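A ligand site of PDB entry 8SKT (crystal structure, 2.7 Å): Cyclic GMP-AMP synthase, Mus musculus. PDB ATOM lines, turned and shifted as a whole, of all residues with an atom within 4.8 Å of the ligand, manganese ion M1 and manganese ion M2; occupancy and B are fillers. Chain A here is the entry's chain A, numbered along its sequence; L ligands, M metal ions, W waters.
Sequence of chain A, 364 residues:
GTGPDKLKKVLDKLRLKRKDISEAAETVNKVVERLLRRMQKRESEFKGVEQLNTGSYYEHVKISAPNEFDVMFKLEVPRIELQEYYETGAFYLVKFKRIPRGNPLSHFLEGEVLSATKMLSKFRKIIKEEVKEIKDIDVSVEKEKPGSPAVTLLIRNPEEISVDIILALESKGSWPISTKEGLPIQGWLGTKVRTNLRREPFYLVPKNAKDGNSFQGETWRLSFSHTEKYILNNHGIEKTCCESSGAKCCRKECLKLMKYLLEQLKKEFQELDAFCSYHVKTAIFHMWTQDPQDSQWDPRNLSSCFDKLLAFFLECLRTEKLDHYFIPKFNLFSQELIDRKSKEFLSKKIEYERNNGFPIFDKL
OE2 of Glu 68 is bound to manganese ion M2 (2.2 Å). Manganese ion M2 is bound by the side-chain carboxylate (OD1) of Asp 70 (2.2 Å). The side-chain carboxylate (OD2) of Asp 164 is bound to manganese ion M2 (2.3 Å). O8 of the ligand is bound to manganese ion M2, at 2.5 Å. Manganese ion M2 has four donor atoms within binding distance.
CA of Gly 55 touches O5 of the ligand, 3.4 Å away. CE2 of Tyr 278 touches C9 of the ligand, at 3.5 Å. Within 4 Å of the ligand: Gly 55, Ser 56, Glu 68, Asp 70, Arg 221, Ser 225, Glu 228, Lys 259, Ser 277, Tyr 278 and Lys 281. The nearest printed residue that does not touch the ligand is Lys 62 (4.1 Å).
OG of Ser 56 touches manganese ion M1, at 3.2 Å. Within 4 Å of manganese ion M1: Ser 56, Glu 68 and Asp 70. The nearest printed residue that does not touch manganese ion M1 is Gly 55 (4.8 Å).
Manganese ion M1 is bound by OE1 of Glu 68, 2.2 Å away. Manganese ion M1 is bound by OD2 of Asp 70, at 2.3 Å. O2 of the ligand is bound to manganese ion M1 (2.3 Å). O5 of the ligand is bound to manganese ion M1, at 2.4 Å. O8 of the ligand binds manganese ion M1. Manganese ion M1 has five donor atoms within binding distance.
OE1 of Glu 228 is in salt-bridge range of NZ of Lys 281. The side-chain carboxylate (OE2) of Glu 228 lies within hydrogen-bond range of the side-chain hydroxyl (OH) of Tyr 278 (2.6 Å). The backbone NH of Lys 62 is in hydrogen-bond range of the backbone carbonyl oxygen of Ser 56 (3.3 Å). NZ of Lys 281 is in salt-bridge range of OE2 of Glu 59 (2.7 Å). N of Tyr 278 sits close to SG of Cys 276 (3.7 Å).
Water W5 lies within hydrogen-bond range of O1 of the ligand, OE2 of Glu 263 and NZ of Lys 62. Water W4 lies within hydrogen-bond range of O4 of the ligand (2.7 Å), OG of Ser 277 (3.0 Å) and N of Tyr 278 (3.1 Å). Water W2 lies within hydrogen-bond range of OE1 of Glu 59 (2.5 Å) and O4 of the ligand (2.8 Å). Water W3 lies within hydrogen-bond range of an oxygen (O7) of the ligand (3.0 Å), the side-chain hydroxyl (OG) of Ser 277 (3.0 Å), the backbone NH (N) of Tyr 278 (3.0 Å) and the side-chain sulfur (SG) of Cys 276 (3.4 Å). Water W1 bridges N of Asp 70 (2.9 Å) and N of Ser 56 (3.4 Å).
The side-chain carboxylate of Glu 228 sits at hydrogen-bond distance from an oxygen (O13) of the ligand. The side-chain hydroxyl of Ser 225 sits at hydrogen-bond distance from an oxygen (O13) of the ligand. O3 of the ligand lies within hydrogen-bond range of OG of Ser 277 (2.7 Å). N of Ser 56 lies close to O5 of the ligand, at 2.8 Å. OG of Ser 56 lies within hydrogen-bond range of O1 of the ligand (2.8 Å). An oxygen (O1) of the ligand lies within salt-bridge range of the side-chain amino group of Lys 259 (2.9 Å). The guanidinium group (NH2) of Arg 221 sits at hydrogen-bond distance from a nitrogen (N5) of the ligand, 3.0 Å away. O12 of the ligand is in hydrogen-bond range of NZ of Lys 281.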
ATOM      1  N   GLY A  55     -13.521  28.686  -0.527  1.00  0.00           N
ATOM      2  CA  GLY A  55     -12.637  29.172   0.485  1.00  0.00           C
ATOM      3  C   GLY A  55     -12.215  30.599   0.255  1.00  0.00           C
ATOM      4  O   GLY A  55     -12.707  31.303  -0.628  1.00  0.00           O
ATOM      5  N   SER A  56     -11.252  31.029   1.084  1.00  0.00           N
ATOM      6  CA  SER A  56     -11.003  32.454   1.219  1.00  0.00           C
ATOM      7  C   SER A  56     -10.578  33.064  -0.103  1.00  0.00           C
ATOM      8  O   SER A  56     -11.050  34.147  -0.472  1.00  0.00           O
ATOM      9  CB  SER A  56      -9.937  32.720   2.301  1.00  0.00           C
ATOM     10  OG  SER A  56      -8.771  31.927   2.112  1.00  0.00           O
ATOM     11  N   GLU A  59     -13.320  33.766  -2.355  1.00  0.00           N
ATOM     12  CA  GLU A  59     -14.291  34.688  -1.802  1.00  0.00           C
ATOM     13  C   GLU A  59     -13.749  36.108  -1.738  1.00  0.00           C
ATOM     14  O   GLU A  59     -14.505  37.032  -1.422  1.00  0.00           O
ATOM     15  CB  GLU A  59     -14.740  34.200  -0.431  1.00  0.00           C
ATOM     16  CG  GLU A  59     -15.538  32.904  -0.445  1.00  0.00           C
ATOM     17  CD  GLU A  59     -15.516  32.166   0.908  1.00  0.00           C
ATOM     18  OE1 GLU A  59     -14.628  32.431   1.746  1.00  0.00           O
ATOM     19  OE2 GLU A  59     -16.427  31.350   1.169  1.00  0.00           O
ATOM     20  N   LYS A  62      -9.163  36.073   1.402  1.00  0.00           N
ATOM     21  CA  LYS A  62      -7.810  35.615   1.702  1.00  0.00           C
ATOM     22  C   LYS A  62      -6.888  36.791   2.015  1.00  0.00           C
ATOM     23  O   LYS A  62      -6.843  37.758   1.258  1.00  0.00           O
ATOM     24  CB  LYS A  62      -7.278  34.823   0.512  1.00  0.00           C
ATOM     25  CG  LYS A  62      -5.820  34.477   0.608  1.00  0.00           C
ATOM     26  CD  LYS A  62      -5.616  33.256   1.479  1.00  0.00           C
ATOM     27  CE  LYS A  62      -4.478  33.527   2.411  1.00  0.00           C
ATOM     28  NZ  LYS A  62      -3.929  32.320   3.058  1.00  0.00           N
ATOM     29  N   GLU A  68      -2.704  29.928   0.369  1.00  0.00           N
ATOM     30  CA  GLU A  68      -3.502  28.741   0.670  1.00  0.00           C
ATOM     31  C   GLU A  68      -4.768  28.783  -0.173  1.00  0.00           C
ATOM     32  O   GLU A  68      -5.493  29.779  -0.160  1.00  0.00           O
ATOM     33  CB  GLU A  68      -3.833  28.648   2.156  1.00  0.00           C
ATOM     34  CG  GLU A  68      -4.137  27.253   2.609  1.00  0.00           C
ATOM     35  CD  GLU A  68      -5.636  26.981   2.643  1.00  0.00           C
ATOM     36  OE1 GLU A  68      -6.383  27.843   2.145  1.00  0.00           O
ATOM     37  OE2 GLU A  68      -6.057  25.912   3.170  1.00  0.00           O
ATOM     38  N   ASP A  70      -8.229  26.439  -1.581  1.00  0.00           N
ATOM     39  CA  ASP A  70      -9.036  25.257  -1.289  1.00  0.00           C
ATOM     40  C   ASP A  70      -9.876  24.930  -2.515  1.00  0.00           C
ATOM     41  O   ASP A  70     -10.568  25.796  -3.041  1.00  0.00           O
ATOM     42  CB  ASP A  70      -9.927  25.450  -0.079  1.00  0.00           C
ATOM     43  CG  ASP A  70      -9.224  26.120   1.072  1.00  0.00           C
ATOM     44  OD1 ASP A  70      -8.338  25.507   1.717  1.00  0.00           O
ATOM     45  OD2 ASP A  70      -9.560  27.283   1.348  1.00  0.00           O
ATOM     46  N   ASP A 164      -5.537  22.616  -0.653  1.00  0.00           N
ATOM     47  CA  ASP A 164      -6.323  21.533  -0.113  1.00  0.00           C
ATOM     48  C   ASP A 164      -7.200  20.980  -1.222  1.00  0.00           C
ATOM     49  O   ASP A 164      -8.150  21.641  -1.653  1.00  0.00           O
ATOM     50  CB  ASP A 164      -7.153  22.030   1.064  1.00  0.00           C
ATOM     51  CG  ASP A 164      -6.329  22.175   2.317  1.00  0.00           C
ATOM     52  OD1 ASP A 164      -5.378  21.381   2.502  1.00  0.00           O
ATOM     53  OD2 ASP A 164      -6.637  23.086   3.109  1.00  0.00           O
ATOM     54  N   ARG A 221     -19.201  14.186   6.676  1.00  0.00           N
ATOM     55  CA  ARG A 221     -19.585  15.482   7.242  1.00  0.00           C
ATOM     56  C   ARG A 221     -20.165  16.378   6.142  1.00  0.00           C
ATOM     57  O   ARG A 221     -19.633  16.436   5.025  1.00  0.00           O
ATOM     58  CB  ARG A 221     -18.375  16.175   7.894  1.00  0.00           C
ATOM     59  CG  ARG A 221     -18.678  17.456   8.670  1.00  0.00           C
ATOM     60  CD  ARG A 221     -17.466  18.397   8.732  1.00  0.00           C
ATOM     61  NE  ARG A 221     -17.549  19.446   7.711  1.00  0.00           N
ATOM     62  CZ  ARG A 221     -16.524  19.880   6.985  1.00  0.00           C
ATOM     63  NH1 ARG A 221     -15.299  19.401   7.132  1.00  0.00           N
ATOM     64  NH2 ARG A 221     -16.739  20.836   6.068  1.00  0.00           N
ATOM     65  N   SER A 225     -19.520  24.834   1.631  1.00  0.00           N
ATOM     66  CA  SER A 225     -18.573  25.781   1.072  1.00  0.00           C
ATOM     67  C   SER A 225     -19.149  26.487  -0.143  1.00  0.00           C
ATOM     68  O   SER A 225     -18.844  27.658  -0.386  1.00  0.00           O
ATOM     69  CB  SER A 225     -17.289  25.070   0.670  1.00  0.00           C
ATOM     70  OG  SER A 225     -16.449  24.877   1.778  1.00  0.00           O
ATOM     71  N   GLU A 228     -21.561  29.155   1.077  1.00  0.00           N
ATOM     72  CA  GLU A 228     -20.823  30.230   1.718  1.00  0.00           C
ATOM     73  C   GLU A 228     -20.120  31.111   0.699  1.00  0.00           C
ATOM     74  O   GLU A 228     -20.057  32.334   0.852  1.00  0.00           O
ATOM     75  CB  GLU A 228     -19.836  29.634   2.709  1.00  0.00           C
ATOM     76  CG  GLU A 228     -20.478  28.734   3.734  1.00  0.00           C
ATOM     77  CD  GLU A 228     -19.462  27.914   4.454  1.00  0.00           C
ATOM     78  OE1 GLU A 228     -18.262  28.077   4.146  1.00  0.00           O
ATOM     79  OE2 GLU A 228     -19.830  27.137   5.363  1.00  0.00           O
ATOM     80  N   LYS A 259     -10.217  37.579  10.907  1.00  0.00           N
ATOM     81  CA  LYS A 259      -9.356  36.495  10.472  1.00  0.00           C
ATOM     82  C   LYS A 259      -7.925  36.737  10.918  1.00  0.00           C
ATOM     83  O   LYS A 259      -7.221  35.818  11.382  1.00  0.00           O
ATOM     84  CB  LYS A 259      -9.395  36.374   8.951  1.00  0.00           C
ATOM     85  CG  LYS A 259     -10.508  35.553   8.378  1.00  0.00           C
ATOM     86  CD  LYS A 259     -10.577  35.821   6.876  1.00  0.00           C
ATOM     87  CE  LYS A 259      -9.447  35.136   6.129  1.00  0.00           C
ATOM     88  NZ  LYS A 259      -9.769  33.697   5.877  1.00  0.00           N
ATOM     89  N   GLU A 263      -5.427  34.669  13.265  1.00  0.00           N
ATOM     90  CA  GLU A 263      -4.185  34.148  12.675  1.00  0.00           C
ATOM     91  C   GLU A 263      -2.955  34.593  13.470  1.00  0.00           C
ATOM     92  O   GLU A 263      -2.120  33.762  13.839  1.00  0.00           O
ATOM     93  CB  GLU A 263      -4.055  34.592  11.211  1.00  0.00           C
ATOM     94  CG  GLU A 263      -4.781  33.710  10.215  1.00  0.00           C
ATOM     95  CD  GLU A 263      -4.423  34.016   8.750  1.00  0.00           C
ATOM     96  OE1 GLU A 263      -3.250  34.387   8.492  1.00  0.00           O
ATOM     97  OE2 GLU A 263      -5.287  33.849   7.849  1.00  0.00           O
ATOM     98  N   CYS A 276     -10.022  27.793  14.578  1.00  0.00           N
ATOM     99  CA  CYS A 276      -9.693  27.906  13.169  1.00  0.00           C
ATOM    100  C   CYS A 276     -10.495  29.065  12.608  1.00  0.00           C
ATOM    101  O   CYS A 276     -11.384  29.612  13.269  1.00  0.00           O
ATOM    102  CB  CYS A 276      -9.981  26.602  12.422  1.00  0.00           C
ATOM    103  SG  CYS A 276     -11.724  26.196  12.368  1.00  0.00           S
ATOM    104  N   SER A 277     -10.201  29.426  11.363  1.00  0.00           N
ATOM    105  CA  SER A 277     -10.849  30.593  10.788  1.00  0.00           C
ATOM    106  C   SER A 277     -12.324  30.342  10.504  1.00  0.00           C
ATOM    107  O   SER A 277     -13.096  31.308  10.427  1.00  0.00           O
ATOM    108  CB  SER A 277     -10.141  31.032   9.522  1.00  0.00           C
ATOM    109  OG  SER A 277     -10.158  29.987   8.572  1.00  0.00           O
ATOM    110  N   TYR A 278     -12.727  29.079  10.334  1.00  0.00           N
ATOM    111  CA  TYR A 278     -14.139  28.817  10.112  1.00  0.00           C
ATOM    112  C   TYR A 278     -14.958  29.273  11.298  1.00  0.00           C
ATOM    113  O   TYR A 278     -16.155  29.567  11.156  1.00  0.00           O
ATOM    114  CB  TYR A 278     -14.389  27.338   9.862  1.00  0.00           C
ATOM    115  CG  TYR A 278     -15.813  27.067   9.372  1.00  0.00           C
ATOM    116  CD1 TYR A 278     -16.220  27.527   8.121  1.00  0.00           C
ATOM    117  CD2 TYR A 278     -16.733  26.372  10.155  1.00  0.00           C
ATOM    118  CE1 TYR A 278     -17.498  27.300   7.653  1.00  0.00           C
ATOM    119  CE2 TYR A 278     -18.041  26.138   9.690  1.00  0.00           C
ATOM    120  CZ  TYR A 278     -18.406  26.603   8.423  1.00  0.00           C
ATOM    121  OH  TYR A 278     -19.664  26.373   7.893  1.00  0.00           O
ATOM    122  N   LYS A 281     -15.563  32.770  10.587  1.00  0.00           N
ATOM    123  CA  LYS A 281     -16.474  32.855   9.443  1.00  0.00           C
ATOM    124  C   LYS A 281     -17.905  32.640   9.898  1.00  0.00           C
ATOM    125  O   LYS A 281     -18.823  33.379   9.503  1.00  0.00           O
ATOM    126  CB  LYS A 281     -16.112  31.822   8.382  1.00  0.00           C
ATOM    127  CG  LYS A 281     -16.665  32.115   7.006  1.00  0.00           C
ATOM    128  CD  LYS A 281     -16.315  30.972   6.062  1.00  0.00           C
ATOM    129  CE  LYS A 281     -16.269  31.430   4.612  1.00  0.00           C
ATOM    130  NZ  LYS A 281     -16.616  30.313   3.660  1.00  0.00           N
ATOM    131  N   HIS A 324     -23.351  26.123  14.262  1.00  0.00           N
ATOM    132  CA  HIS A 324     -23.171  26.035  12.826  1.00  0.00           C
ATOM    133  C   HIS A 324     -24.250  26.842  12.127  1.00  0.00           C
ATOM    134  O   HIS A 324     -25.430  26.774  12.481  1.00  0.00           O
ATOM    135  CB  HIS A 324     -23.234  24.559  12.401  1.00  0.00           C
ATOM    136  CG  HIS A 324     -22.567  24.281  11.092  1.00  0.00           C
ATOM    137  ND1 HIS A 324     -23.061  24.732   9.887  1.00  0.00           N
ATOM    138  CD2 HIS A 324     -21.441  23.578  10.803  1.00  0.00           C
ATOM    139  CE1 HIS A 324     -22.265  24.318   8.916  1.00  0.00           C
ATOM    140  NE2 HIS A 324     -21.286  23.609   9.438  1.00  0.00           N
HETATM  141  P1  LIG L   1      -8.353  30.755   5.268  1.00  0.00           P
HETATM  142  O1  LIG L   1      -7.763  32.009   4.707  1.00  0.00           O
HETATM  143  O2  LIG L   1      -7.805  29.504   4.603  1.00  0.00           O
HETATM  144  O3  LIG L   1      -8.168  30.584   6.779  1.00  0.00           O
HETATM  145  P2  LIG L   1     -10.970  29.600   4.572  1.00  0.00           P
HETATM  146  O4  LIG L   1     -12.403  29.954   4.783  1.00  0.00           O
HETATM  147  O5  LIG L   1     -10.587  29.219   3.156  1.00  0.00           O
HETATM  148  O6  LIG L   1      -9.923  30.661   5.038  1.00  0.00           O
HETATM  149  P3  LIG L   1     -10.075  26.922   5.253  1.00  0.00           P
HETATM  150  O7  LIG L   1      -9.745  26.280   6.536  1.00  0.00           O
HETATM  151  O8  LIG L   1      -9.033  27.073   4.148  1.00  0.00           O
HETATM  152  O9  LIG L   1     -10.580  28.362   5.488  1.00  0.00           O
HETATM  153  O10 LIG L   1     -11.384  26.122   4.835  1.00  0.00           O
HETATM  154  C1  LIG L   1     -11.889  26.127   3.491  1.00  0.00           C
HETATM  155  C2  LIG L   1     -13.392  26.034   3.568  1.00  0.00           C
HETATM  156  O11 LIG L   1     -13.818  24.729   4.061  1.00  0.00           O
HETATM  157  C3  LIG L   1     -14.050  27.028   4.518  1.00  0.00           C
HETATM  158  O12 LIG L   1     -14.275  28.269   3.857  1.00  0.00           O
HETATM  159  C4  LIG L   1     -15.382  26.344   4.854  1.00  0.00           C
HETATM  160  O13 LIG L   1     -16.364  26.618   3.864  1.00  0.00           O
HETATM  161  C5  LIG L   1     -14.964  24.861   4.887  1.00  0.00           C
HETATM  162  N1  LIG L   1     -14.613  24.437   6.232  1.00  0.00           N
HETATM  163  C6  LIG L   1     -13.391  24.557   6.839  1.00  0.00           C
HETATM  164  N2  LIG L   1     -13.358  24.137   8.078  1.00  0.00           N
HETATM  165  C7  LIG L   1     -14.657  23.724   8.316  1.00  0.00           C
HETATM  166  C8  LIG L   1     -15.290  23.171   9.446  1.00  0.00           C
HETATM  167  N3  LIG L   1     -14.666  22.923  10.602  1.00  0.00           N
HETATM  168  N4  LIG L   1     -16.608  22.868   9.353  1.00  0.00           N
HETATM  169  C9  LIG L   1     -17.242  23.116   8.196  1.00  0.00           C
HETATM  170  N5  LIG L   1     -16.750  23.645   7.071  1.00  0.00           N
HETATM  171  C10 LIG L   1     -15.444  23.916   7.189  1.00  0.00           C
HETATM  172 MN    MN M   1      -8.340  28.771   2.518  1.00  0.00          MN
HETATM  173 MN    MN M   2      -7.892  24.858   3.815  1.00  0.00          MN
HETATM  174  O   HOH W   1      -9.232  29.009  -0.849  1.00  0.00           O
HETATM  175  O   HOH W   2     -13.357  32.420   3.953  1.00  0.00           O
HETATM  176  O   HOH W   3     -10.735  27.139   9.202  1.00  0.00           O
HETATM  177  O   HOH W   4     -12.923  29.971   7.410  1.00  0.00           O
HETATM  178  O   HOH W   5      -6.083  33.985   4.767  1.00  0.00           O
